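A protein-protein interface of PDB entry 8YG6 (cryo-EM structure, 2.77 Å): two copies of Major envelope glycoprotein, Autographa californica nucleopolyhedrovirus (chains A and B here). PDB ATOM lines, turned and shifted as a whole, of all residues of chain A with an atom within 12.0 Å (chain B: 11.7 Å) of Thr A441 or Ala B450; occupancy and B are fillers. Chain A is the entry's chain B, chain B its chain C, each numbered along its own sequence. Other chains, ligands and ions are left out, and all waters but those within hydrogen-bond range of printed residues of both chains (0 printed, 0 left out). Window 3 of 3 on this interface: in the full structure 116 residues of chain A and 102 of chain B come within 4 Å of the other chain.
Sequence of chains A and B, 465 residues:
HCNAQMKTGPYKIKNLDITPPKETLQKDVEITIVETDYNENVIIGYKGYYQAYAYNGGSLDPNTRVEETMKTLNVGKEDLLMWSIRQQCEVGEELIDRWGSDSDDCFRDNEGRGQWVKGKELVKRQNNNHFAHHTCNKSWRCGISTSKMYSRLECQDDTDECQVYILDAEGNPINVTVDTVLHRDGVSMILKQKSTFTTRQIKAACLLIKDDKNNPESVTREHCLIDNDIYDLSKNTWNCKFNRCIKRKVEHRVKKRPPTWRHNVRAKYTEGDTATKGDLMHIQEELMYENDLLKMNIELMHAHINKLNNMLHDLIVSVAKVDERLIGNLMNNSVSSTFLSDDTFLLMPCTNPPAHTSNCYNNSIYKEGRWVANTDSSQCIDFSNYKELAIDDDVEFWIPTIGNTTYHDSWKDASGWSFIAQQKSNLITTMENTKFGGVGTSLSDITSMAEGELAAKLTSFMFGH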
ATOM      1  N   THR A 434       8.379  21.987  35.905  1.00  0.00           N
ATOM      2  CA  THR A 434       7.026  22.210  35.402  1.00  0.00           C
ATOM      3  C   THR A 434       7.016  23.499  34.592  1.00  0.00           C
ATOM      4  O   THR A 434       7.045  24.600  35.145  1.00  0.00           O
ATOM      5  CB  THR A 434       6.030  22.274  36.551  1.00  0.00           C
ATOM      6  OG1 THR A 434       6.000  21.011  37.228  1.00  0.00           O
ATOM      7  CG2 THR A 434       4.637  22.594  36.031  1.00  0.00           C
ATOM      8  N   LYS A 435       6.968  23.367  33.267  1.00  0.00           N
ATOM      9  CA  LYS A 435       6.903  24.519  32.372  1.00  0.00           C
ATOM     10  C   LYS A 435       5.503  25.134  32.428  1.00  0.00           C
ATOM     11  O   LYS A 435       4.617  24.827  31.633  1.00  0.00           O
ATOM     12  CB  LYS A 435       7.277  24.113  30.951  1.00  0.00           C
ATOM     13  CG  LYS A 435       8.714  23.654  30.792  1.00  0.00           C
ATOM     14  CD  LYS A 435       8.976  23.162  29.380  1.00  0.00           C
ATOM     15  CE  LYS A 435      10.419  22.714  29.209  1.00  0.00           C
ATOM     16  NZ  LYS A 435      10.676  22.187  27.841  1.00  0.00           N
ATOM     17  N   PHE A 436       5.321  26.003  33.422  1.00  0.00           N
ATOM     18  CA  PHE A 436       4.029  26.629  33.667  1.00  0.00           C
ATOM     19  C   PHE A 436       3.509  27.315  32.409  1.00  0.00           C
ATOM     20  O   PHE A 436       4.224  28.063  31.736  1.00  0.00           O
ATOM     21  CB  PHE A 436       4.142  27.628  34.823  1.00  0.00           C
ATOM     22  CG  PHE A 436       5.387  28.472  34.779  1.00  0.00           C
ATOM     23  CD1 PHE A 436       5.420  29.652  34.053  1.00  0.00           C
ATOM     24  CD2 PHE A 436       6.523  28.082  35.465  1.00  0.00           C
ATOM     25  CE1 PHE A 436       6.566  30.425  34.014  1.00  0.00           C
ATOM     26  CE2 PHE A 436       7.671  28.851  35.428  1.00  0.00           C
ATOM     27  CZ  PHE A 436       7.693  30.024  34.703  1.00  0.00           C
ATOM     28  N   GLY A 437       2.248  27.040  32.093  1.00  0.00           N
ATOM     29  CA  GLY A 437       1.650  27.563  30.878  1.00  0.00           C
ATOM     30  C   GLY A 437       0.372  26.813  30.556  1.00  0.00           C
ATOM     31  O   GLY A 437      -0.151  26.068  31.387  1.00  0.00           O
ATOM     32  N   GLY A 438      -0.116  27.021  29.336  1.00  0.00           N
ATOM     33  CA  GLY A 438      -1.353  26.396  28.909  1.00  0.00           C
ATOM     34  C   GLY A 438      -1.167  25.071  28.195  1.00  0.00           C
ATOM     35  O   GLY A 438      -1.740  24.853  27.125  1.00  0.00           O
ATOM     36  N   VAL A 439      -0.364  24.176  28.776  1.00  0.00           N
ATOM     37  CA  VAL A 439      -0.108  22.863  28.205  1.00  0.00           C
ATOM     38  C   VAL A 439      -0.567  21.737  29.124  1.00  0.00           C
ATOM     39  O   VAL A 439      -1.120  20.736  28.654  1.00  0.00           O
ATOM     40  CB  VAL A 439       1.381  22.692  27.833  1.00  0.00           C
ATOM     41  CG1 VAL A 439       1.741  23.622  26.685  1.00  0.00           C
ATOM     42  CG2 VAL A 439       2.276  22.975  29.029  1.00  0.00           C
ATOM     43  N   GLY A 440      -0.343  21.869  30.429  1.00  0.00           N
ATOM     44  CA  GLY A 440      -0.785  20.846  31.363  1.00  0.00           C
ATOM     45  C   GLY A 440      -2.301  20.762  31.398  1.00  0.00           C
ATOM     46  O   GLY A 440      -2.985  21.740  31.720  1.00  0.00           O
ATOM     47  N   THR A 441      -2.835  19.583  31.068  1.00  0.00           N
ATOM     48  CA  THR A 441      -4.281  19.414  30.971  1.00  0.00           C
ATOM     49  C   THR A 441      -4.761  18.097  31.574  1.00  0.00           C
ATOM     50  O   THR A 441      -5.952  17.777  31.466  1.00  0.00           O
ATOM     51  CB  THR A 441      -4.736  19.510  29.515  1.00  0.00           C
ATOM     52  OG1 THR A 441      -6.154  19.307  29.439  1.00  0.00           O
ATOM     53  CG2 THR A 441      -4.020  18.476  28.665  1.00  0.00           C
ATOM     54  N   SER A 442      -3.875  17.325  32.204  1.00  0.00           N
ATOM     55  CA  SER A 442      -4.277  16.077  32.843  1.00  0.00           C
ATOM     56  C   SER A 442      -4.974  16.296  34.179  1.00  0.00           C
ATOM     57  O   SER A 442      -5.250  15.317  34.881  1.00  0.00           O
ATOM     58  CB  SER A 442      -3.057  15.174  33.040  1.00  0.00           C
ATOM     59  OG  SER A 442      -3.446  13.867  33.419  1.00  0.00           O
ATOM     60  N   LEU A 443      -5.258  17.545  34.540  1.00  0.00           N
ATOM     61  CA  LEU A 443      -5.903  17.879  35.800  1.00  0.00           C
ATOM     62  C   LEU A 443      -7.415  18.029  35.688  1.00  0.00           C
ATOM     63  O   LEU A 443      -8.072  18.263  36.708  1.00  0.00           O
ATOM     64  CB  LEU A 443      -5.313  19.179  36.371  1.00  0.00           C
ATOM     65  CG  LEU A 443      -5.714  20.501  35.706  1.00  0.00           C
ATOM     66  CD1 LEU A 443      -5.361  21.667  36.608  1.00  0.00           C
ATOM     67  CD2 LEU A 443      -5.058  20.683  34.344  1.00  0.00           C
ATOM     68  N   SER A 444      -7.977  17.904  34.490  1.00  0.00           N
ATOM     69  CA  SER A 444      -9.406  18.095  34.277  1.00  0.00           C
ATOM     70  C   SER A 444     -10.225  16.843  34.554  1.00  0.00           C
ATOM     71  O   SER A 444     -11.445  16.864  34.359  1.00  0.00           O
ATOM     72  CB  SER A 444      -9.663  18.572  32.843  1.00  0.00           C
ATOM     73  OG  SER A 444     -11.002  19.009  32.687  1.00  0.00           O
ATOM     74  N   ASP A 445      -9.594  15.759  35.002  1.00  0.00           N
ATOM     75  CA  ASP A 445     -10.318  14.527  35.293  1.00  0.00           C
ATOM     76  C   ASP A 445      -9.940  13.979  36.663  1.00  0.00           C
ATOM     77  O   ASP A 445      -9.262  14.655  37.443  1.00  0.00           O
ATOM     78  CB  ASP A 445     -10.065  13.485  34.196  1.00  0.00           C
ATOM     79  CG  ASP A 445      -8.588  13.262  33.920  1.00  0.00           C
ATOM     80  OD1 ASP A 445      -7.756  13.487  34.824  1.00  0.00           O
ATOM     81  OD2 ASP A 445      -8.258  12.856  32.786  1.00  0.00           O
ATOM     82  N   ILE A 446     -10.373  12.757  36.963  1.00  0.00           N
ATOM     83  CA  ILE A 446     -10.165  12.159  38.275  1.00  0.00           C
ATOM     84  C   ILE A 446      -9.144  11.037  38.111  1.00  0.00           C
ATOM     85  O   ILE A 446      -8.765  10.698  36.984  1.00  0.00           O
ATOM     86  CB  ILE A 446     -11.505  11.662  38.859  1.00  0.00           C
ATOM     87  CG1 ILE A 446     -12.536  12.787  38.812  1.00  0.00           C
ATOM     88  CG2 ILE A 446     -11.367  11.251  40.318  1.00  0.00           C
ATOM     89  CD1 ILE A 446     -12.146  14.012  39.611  1.00  0.00           C
ATOM     90  N   THR A 447      -8.684  10.459  39.224  1.00  0.00           N
ATOM     91  CA  THR A 447      -7.619   9.461  39.199  1.00  0.00           C
ATOM     92  C   THR A 447      -7.998   8.184  38.460  1.00  0.00           C
ATOM     93  O   THR A 447      -7.160   7.280  38.362  1.00  0.00           O
ATOM     94  CB  THR A 447      -7.207   9.109  40.630  1.00  0.00           C
ATOM     95  OG1 THR A 447      -8.375   8.858  41.420  1.00  0.00           O
ATOM     96  CG2 THR A 447      -6.417  10.251  41.253  1.00  0.00           C
ATOM     97  N   SER A 448      -9.227   8.078  37.948  1.00  0.00           N
ATOM     98  CA  SER A 448      -9.632   6.876  37.226  1.00  0.00           C
ATOM     99  C   SER A 448      -8.792   6.675  35.969  1.00  0.00           C
ATOM    100  O   SER A 448      -8.333   5.563  35.687  1.00  0.00           O
ATOM    101  CB  SER A 448     -11.117   6.957  36.870  1.00  0.00           C
ATOM    102  OG  SER A 448     -11.396   8.138  36.137  1.00  0.00           O
ATOM    103  N   MET A 449      -8.548   7.759  35.228  1.00  0.00           N
ATOM    104  CA  MET A 449      -7.904   7.658  33.921  1.00  0.00           C
ATOM    105  C   MET A 449      -6.500   7.076  34.000  1.00  0.00           C
ATOM    106  O   MET A 449      -5.966   6.638  32.976  1.00  0.00           O
ATOM    107  CB  MET A 449      -7.894   9.040  33.246  1.00  0.00           C
ATOM    108  CG  MET A 449      -6.785  10.012  33.672  1.00  0.00           C
ATOM    109  SD  MET A 449      -5.128   9.722  33.009  1.00  0.00           S
ATOM    110  CE  MET A 449      -5.379  10.112  31.281  1.00  0.00           C
ATOM    111  N   ALA A 450      -5.886   7.064  35.186  1.00  0.00           N
ATOM    112  CA  ALA A 450      -4.567   6.455  35.326  1.00  0.00           C
ATOM    113  C   ALA A 450      -4.607   4.973  34.987  1.00  0.00           C
ATOM    114  O   ALA A 450      -3.716   4.463  34.295  1.00  0.00           O
ATOM    115  CB  ALA A 450      -4.042   6.662  36.746  1.00  0.00           C
ATOM    116  N   GLU A 453      -8.444   3.663  31.262  1.00  0.00           N
ATOM    117  CA  GLU A 453      -8.186   3.635  29.827  1.00  0.00           C
ATOM    118  C   GLU A 453      -6.935   2.831  29.500  1.00  0.00           C
ATOM    119  O   GLU A 453      -6.868   2.180  28.454  1.00  0.00           O
ATOM    120  CB  GLU A 453      -8.073   5.060  29.282  1.00  0.00           C
ATOM    121  CG  GLU A 453      -9.406   5.786  29.148  1.00  0.00           C
ATOM    122  CD  GLU A 453     -10.060   6.096  30.480  1.00  0.00           C
ATOM    123  OE1 GLU A 453      -9.358   6.076  31.511  1.00  0.00           O
ATOM    124  OE2 GLU A 453     -11.281   6.357  30.492  1.00  0.00           O
ATOM    125  N   LEU A 454      -5.938   2.848  30.388  1.00  0.00           N
ATOM    126  CA  LEU A 454      -4.722   2.077  30.152  1.00  0.00           C
ATOM    127  C   LEU A 454      -5.019   0.582  30.095  1.00  0.00           C
ATOM    128  O   LEU A 454      -4.638  -0.110  29.142  1.00  0.00           O
ATOM    129  CB  LEU A 454      -3.688   2.384  31.239  1.00  0.00           C
ATOM    130  CG  LEU A 454      -2.277   1.813  31.060  1.00  0.00           C
ATOM    131  CD1 LEU A 454      -1.242   2.761  31.649  1.00  0.00           C
ATOM    132  CD2 LEU A 454      -2.148   0.425  31.672  1.00  0.00           C
ATOM    133  N   SER B  59     -19.134  13.134  32.164  1.00  0.00           N
ATOM    134  CA  SER B  59     -17.933  13.815  31.612  1.00  0.00           C
ATOM    135  C   SER B  59     -18.122  13.999  30.106  1.00  0.00           C
ATOM    136  O   SER B  59     -19.240  13.744  29.625  1.00  0.00           O
ATOM    137  CB  SER B  59     -16.684  13.033  31.914  1.00  0.00           C
ATOM    138  OG  SER B  59     -15.543  13.664  31.353  1.00  0.00           O
ATOM    139  N   LEU B  60     -17.072  14.423  29.398  1.00  0.00           N
ATOM    140  CA  LEU B  60     -17.164  14.553  27.920  1.00  0.00           C
ATOM    141  C   LEU B  60     -18.530  15.153  27.576  1.00  0.00           C
ATOM    142  O   LEU B  60     -19.120  14.719  26.570  1.00  0.00           O
ATOM    143  CB  LEU B  60     -17.022  13.158  27.296  1.00  0.00           C
ATOM    144  CG  LEU B  60     -15.677  12.444  27.471  1.00  0.00           C
ATOM    145  CD1 LEU B  60     -15.750  11.025  26.927  1.00  0.00           C
ATOM    146  CD2 LEU B  60     -14.565  13.219  26.781  1.00  0.00           C
ATOM    147  N   ASP B  61     -19.027  16.086  28.393  1.00  0.00           N
ATOM    148  CA  ASP B  61     -20.400  16.613  28.170  1.00  0.00           C
ATOM    149  C   ASP B  61     -20.447  18.115  28.450  1.00  0.00           C
ATOM    150  O   ASP B  61     -19.549  18.611  29.150  1.00  0.00           O
ATOM    151  CB  ASP B  61     -21.406  15.897  29.072  1.00  0.00           C
ATOM    152  CG  ASP B  61     -21.210  16.219  30.545  1.00  0.00           C
ATOM    153  OD1 ASP B  61     -20.051  16.199  31.000  1.00  0.00           O
ATOM    154  OD2 ASP B  61     -22.216  16.491  31.219  1.00  0.00           O
ATOM    155  N   GLY B 440       7.585  13.629  35.404  1.00  0.00           N
ATOM    156  CA  GLY B 440       6.538  14.350  34.699  1.00  0.00           C
ATOM    157  C   GLY B 440       6.948  14.640  33.267  1.00  0.00           C
ATOM    158  O   GLY B 440       7.957  15.311  33.017  1.00  0.00           O
ATOM    159  N   THR B 441       6.159  14.138  32.313  1.00  0.00           N
ATOM    160  CA  THR B 441       6.509  14.270  30.904  1.00  0.00           C
ATOM    161  C   THR B 441       5.306  14.611  30.027  1.00  0.00           C
ATOM    162  O   THR B 441       5.440  14.650  28.798  1.00  0.00           O
ATOM    163  CB  THR B 441       7.171  12.989  30.391  1.00  0.00           C
ATOM    164  OG1 THR B 441       7.472  13.127  28.997  1.00  0.00           O
ATOM    165  CG2 THR B 441       6.254  11.797  30.606  1.00  0.00           C
ATOM    166  N   SER B 442       4.139  14.861  30.622  1.00  0.00           N
ATOM    167  CA  SER B 442       2.962  15.241  29.847  1.00  0.00           C
ATOM    168  C   SER B 442       2.996  16.694  29.394  1.00  0.00           C
ATOM    169  O   SER B 442       2.002  17.176  28.842  1.00  0.00           O
ATOM    170  CB  SER B 442       1.694  14.985  30.666  1.00  0.00           C
ATOM    171  OG  SER B 442       0.535  15.101  29.859  1.00  0.00           O
ATOM    172  N   LEU B 443       4.107  17.394  29.618  1.00  0.00           N
ATOM    173  CA  LEU B 443       4.250  18.794  29.249  1.00  0.00           C
ATOM    174  C   LEU B 443       4.912  19.000  27.893  1.00  0.00           C
ATOM    175  O   LEU B 443       5.039  20.148  27.456  1.00  0.00           O
ATOM    176  CB  LEU B 443       5.058  19.545  30.319  1.00  0.00           C
ATOM    177  CG  LEU B 443       6.572  19.306  30.373  1.00  0.00           C
ATOM    178  CD1 LEU B 443       7.240  20.384  31.203  1.00  0.00           C
ATOM    179  CD2 LEU B 443       6.918  17.933  30.932  1.00  0.00           C
ATOM    180  N   SER B 444       5.333  17.930  27.224  1.00  0.00           N
ATOM    181  CA  SER B 444       6.035  18.036  25.952  1.00  0.00           C
ATOM    182  C   SER B 444       5.096  18.146  24.759  1.00  0.00           C
ATOM    183  O   SER B 444       5.571  18.188  23.618  1.00  0.00           O
ATOM    184  CB  SER B 444       6.966  16.833  25.766  1.00  0.00           C
ATOM    185  OG  SER B 444       7.842  17.035  24.671  1.00  0.00           O
ATOM    186  N   ASP B 445       3.785  18.194  24.986  1.00  0.00           N
ATOM    187  CA  ASP B 445       2.829  18.304  23.890  1.00  0.00           C
ATOM    188  C   ASP B 445       1.814  19.406  24.157  1.00  0.00           C
ATOM    189  O   ASP B 445       1.971  20.190  25.097  1.00  0.00           O
ATOM    190  CB  ASP B 445       2.131  16.960  23.650  1.00  0.00           C
ATOM    191  CG  ASP B 445       1.528  16.373  24.915  1.00  0.00           C
ATOM    192  OD1 ASP B 445       1.194  17.134  25.844  1.00  0.00           O
ATOM    193  OD2 ASP B 445       1.386  15.133  24.976  1.00  0.00           O
ATOM    194  N   ILE B 446       0.769  19.475  23.333  1.00  0.00           N
ATOM    195  CA  ILE B 446      -0.220  20.542  23.420  1.00  0.00           C
ATOM    196  C   ILE B 446      -1.514  19.924  23.943  1.00  0.00           C
ATOM    197  O   ILE B 446      -1.613  18.700  24.075  1.00  0.00           O
ATOM    198  CB  ILE B 446      -0.399  21.222  22.047  1.00  0.00           C
ATOM    199  CG1 ILE B 446       0.963  21.639  21.497  1.00  0.00           C
ATOM    200  CG2 ILE B 446      -1.239  22.488  22.148  1.00  0.00           C
ATOM    201  CD1 ILE B 446       1.704  22.626  22.374  1.00  0.00           C
ATOM    202  N   THR B 447      -2.509  20.760  24.253  1.00  0.00           N
ATOM    203  CA  THR B 447      -3.747  20.300  24.873  1.00  0.00           C
ATOM    204  C   THR B 447      -4.555  19.354  23.993  1.00  0.00           C
ATOM    205  O   THR B 447      -5.613  18.888  24.432  1.00  0.00           O
ATOM    206  CB  THR B 447      -4.617  21.502  25.249  1.00  0.00           C
ATOM    207  OG1 THR B 447      -4.690  22.407  24.142  1.00  0.00           O
ATOM    208  CG2 THR B 447      -4.030  22.228  26.451  1.00  0.00           C
ATOM    209  N   SER B 448      -4.098  19.066  22.772  1.00  0.00           N
ATOM    210  CA  SER B 448      -4.835  18.160  21.896  1.00  0.00           C
ATOM    211  C   SER B 448      -4.923  16.761  22.494  1.00  0.00           C
ATOM    212  O   SER B 448      -5.990  16.136  22.491  1.00  0.00           O
ATOM    213  CB  SER B 448      -4.173  18.112  20.519  1.00  0.00           C
ATOM    214  OG  SER B 448      -2.806  17.753  20.628  1.00  0.00           O
ATOM    215  N   MET B 449      -3.813  16.273  23.054  1.00  0.00           N
ATOM    216  CA  MET B 449      -3.732  14.885  23.503  1.00  0.00           C
ATOM    217  C   MET B 449      -4.738  14.563  24.598  1.00  0.00           C
ATOM    218  O   MET B 449      -5.006  13.382  24.846  1.00  0.00           O
ATOM    219  CB  MET B 449      -2.297  14.577  23.958  1.00  0.00           C
ATOM    220  CG  MET B 449      -1.910  15.015  25.378  1.00  0.00           C
ATOM    221  SD  MET B 449      -2.519  14.011  26.752  1.00  0.00           S
ATOM    222  CE  MET B 449      -1.582  12.505  26.514  1.00  0.00           C
ATOM    223  N   ALA B 450      -5.296  15.577  25.264  1.00  0.00           N
ATOM    224  CA  ALA B 450      -6.315  15.321  26.277  1.00  0.00           C
ATOM    225  C   ALA B 450      -7.535  14.645  25.670  1.00  0.00           C
ATOM    226  O   ALA B 450      -8.083  13.698  26.250  1.00  0.00           O
ATOM    227  CB  ALA B 450      -6.716  16.627  26.959  1.00  0.00           C
ATOM    228  N   GLU B 451      -7.977  15.108  24.503  1.00  0.00           N
ATOM    229  CA  GLU B 451      -9.179  14.579  23.878  1.00  0.00           C
ATOM    230  C   GLU B 451      -8.910  13.721  22.648  1.00  0.00           C
ATOM    231  O   GLU B 451      -9.635  12.746  22.432  1.00  0.00           O
ATOM    232  CB  GLU B 451     -10.127  15.728  23.505  1.00  0.00           C
ATOM    233  CG  GLU B 451      -9.551  16.755  22.533  1.00  0.00           C
ATOM    234  CD  GLU B 451      -9.743  16.372  21.078  1.00  0.00           C
ATOM    235  OE1 GLU B 451     -10.622  15.533  20.792  1.00  0.00           O
ATOM    236  OE2 GLU B 451      -9.010  16.909  20.219  1.00  0.00           O
ATOM    237  N   GLY B 452      -7.897  14.052  21.848  1.00  0.00           N
ATOM    238  CA  GLY B 452      -7.677  13.382  20.583  1.00  0.00           C
ATOM    239  C   GLY B 452      -7.472  11.885  20.684  1.00  0.00           C
ATOM    240  O   GLY B 452      -8.297  11.104  20.198  1.00  0.00           O
ATOM    241  N   GLU B 453      -6.369  11.480  21.317  1.00  0.00           N
ATOM    242  CA  GLU B 453      -6.059  10.060  21.424  1.00  0.00           C
ATOM    243  C   GLU B 453      -7.096   9.324  22.263  1.00  0.00           C
ATOM    244  O   GLU B 453      -7.396   8.157  21.998  1.00  0.00           O
ATOM    245  CB  GLU B 453      -4.656   9.867  22.002  1.00  0.00           C
ATOM    246  CG  GLU B 453      -3.528  10.160  21.020  1.00  0.00           C
ATOM    247  CD  GLU B 453      -3.424  11.623  20.641  1.00  0.00           C
ATOM    248  OE1 GLU B 453      -3.974  12.471  21.372  1.00  0.00           O
ATOM    249  OE2 GLU B 453      -2.794  11.921  19.606  1.00  0.00           O
ATOM    250  N   LEU B 454      -7.666   9.992  23.268  1.00  0.00           N
ATOM    251  CA  LEU B 454      -8.687   9.356  24.093  1.00  0.00           C
ATOM    252  C   LEU B 454      -9.918   8.993  23.268  1.00  0.00           C
ATOM    253  O   LEU B 454     -10.385   7.847  23.287  1.00  0.00           O
ATOM    254  CB  LEU B 454      -9.068  10.277  25.257  1.00  0.00           C
ATOM    255  CG  LEU B 454      -9.991   9.710  26.342  1.00  0.00           C
ATOM    256  CD1 LEU B 454      -9.649  10.312  27.697  1.00  0.00           C
ATOM    257  CD2 LEU B 454     -11.457   9.932  26.006  1.00  0.00           C
ATOM    258  N   ALA B 455     -10.450   9.964  22.519  1.00  0.00           N
ATOM    259  CA  ALA B 455     -11.607   9.695  21.674  1.00  0.00           C
ATOM    260  C   ALA B 455     -11.280   8.703  20.568  1.00  0.00           C
ATOM    261  O   ALA B 455     -12.119   7.859  20.229  1.00  0.00           O
ATOM    262  CB  ALA B 455     -12.141  10.997  21.078  1.00  0.00           C
ATOM    263  N   ALA B 456     -10.082   8.795  19.985  1.00  0.00           N
ATOM    264  CA  ALA B 456      -9.711   7.864  18.927  1.00  0.00           C
ATOM    265  C   ALA B 456      -9.629   6.438  19.455  1.00  0.00           C
ATOM    266  O   ALA B 456     -10.084   5.496  18.799  1.00  0.00           O
ATOM    267  CB  ALA B 456      -8.391   8.292  18.290  1.00  0.00           C
ATOM    268  N   LYS B 457      -9.057   6.260  20.649  1.00  0.00           N
ATOM    269  CA  LYS B 457      -9.045   4.944  21.279  1.00  0.00           C
ATOM    270  C   LYS B 457     -10.453   4.455  21.583  1.00  0.00           C
ATOM    271  O   LYS B 457     -10.752   3.270  21.390  1.00  0.00           O
ATOM    272  CB  LYS B 457      -8.211   4.979  22.561  1.00  0.00           C
ATOM    273  CG  LYS B 457      -8.281   3.695  23.371  1.00  0.00           C
ATOM    274  CD  LYS B 457      -7.762   3.888  24.784  1.00  0.00           C
ATOM    275  CE  LYS B 457      -8.539   3.023  25.758  1.00  0.00           C
ATOM    276  NZ  LYS B 457      -8.772   1.658  25.219  1.00  0.00           N
ATOM    277  N   LEU B 458     -11.325   5.346  22.062  1.00  0.00           N
ATOM    278  CA  LEU B 458     -12.706   4.955  22.329  1.00  0.00           C
ATOM    279  C   LEU B 458     -13.375   4.432  21.064  1.00  0.00           C
ATOM    280  O   LEU B 458     -13.972   3.348  21.063  1.00  0.00           O
ATOM    281  CB  LEU B 458     -13.480   6.141  22.905  1.00  0.00           C
ATOM    282  CG  LEU B 458     -13.028   6.647  24.273  1.00  0.00           C
ATOM    283  CD1 LEU B 458     -13.792   7.907  24.639  1.00  0.00           C
ATOM    284  CD2 LEU B 458     -13.208   5.578  25.340  1.00  0.00           C
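Among the printed residues, merely in contact across the chains: Lys A435 with Leu B443 (3.6 Å), Gly A438 with Thr B447 (3.5 Å), Val A439 with Asp B445 (3.8 Å), Val A439 with Thr B447 (3.9 Å), Thr A441 with Ala B450 (3.7 Å) and Glu A453 with Lys B457 (3.3 Å).
Thr A441 touches Ala B450, but with the chains exchanged Ala A450 does not touch Thr B441 (12.9 Å).
Of the 6 pairs that touch across the chains among the printed residues, none has its exchanged pair printed and touching as well.
Thr A434 touches none of the printed residues of chain B.
Printed residues of chain B within 4 Å of Gly A438: Thr B447 (3.5 Å).
Val A439 touches two residues of chain B.
No residue of chain B comes within 4 Å of Gly A440.
Thr A441 touches just one residue of chain B: Ala B450 (3.7 Å).
No residue of chain B comes within 4 Å of Leu A443.
No residue of chain B comes within 4 Å of Asp A445.
Printed residues of chain A within 4 Å of Leu B443: Lys A435 (3.6 Å).
Of chain A, only Gly A438 and Val A439 come within 4 Å of Thr B447.
No residue of chain A comes within 4 Å of Ser B448.
No residue of chain A comes within 4 Å of Glu B451.
No residue of chain A comes within 4 Å of Gly B452.
No residue of chain A comes within 4 Å of Glu B453.
Of the printed residues of chain A, Lys B457 touches Glu A453.
The nearest residue of chain B that does not touch Thr A441 is Thr B447 (4.2 Å).
Along chain A the printed residues that touch a printed residue of chain B span positions 435 to 453.
Of the 22 printed residues of chain B, 5 touch a printed residue of chain A.
Hydrophobic or aromatic side chains of chain B within 4 Å of the printed part of chain A: Leu B443 and Ala B450.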
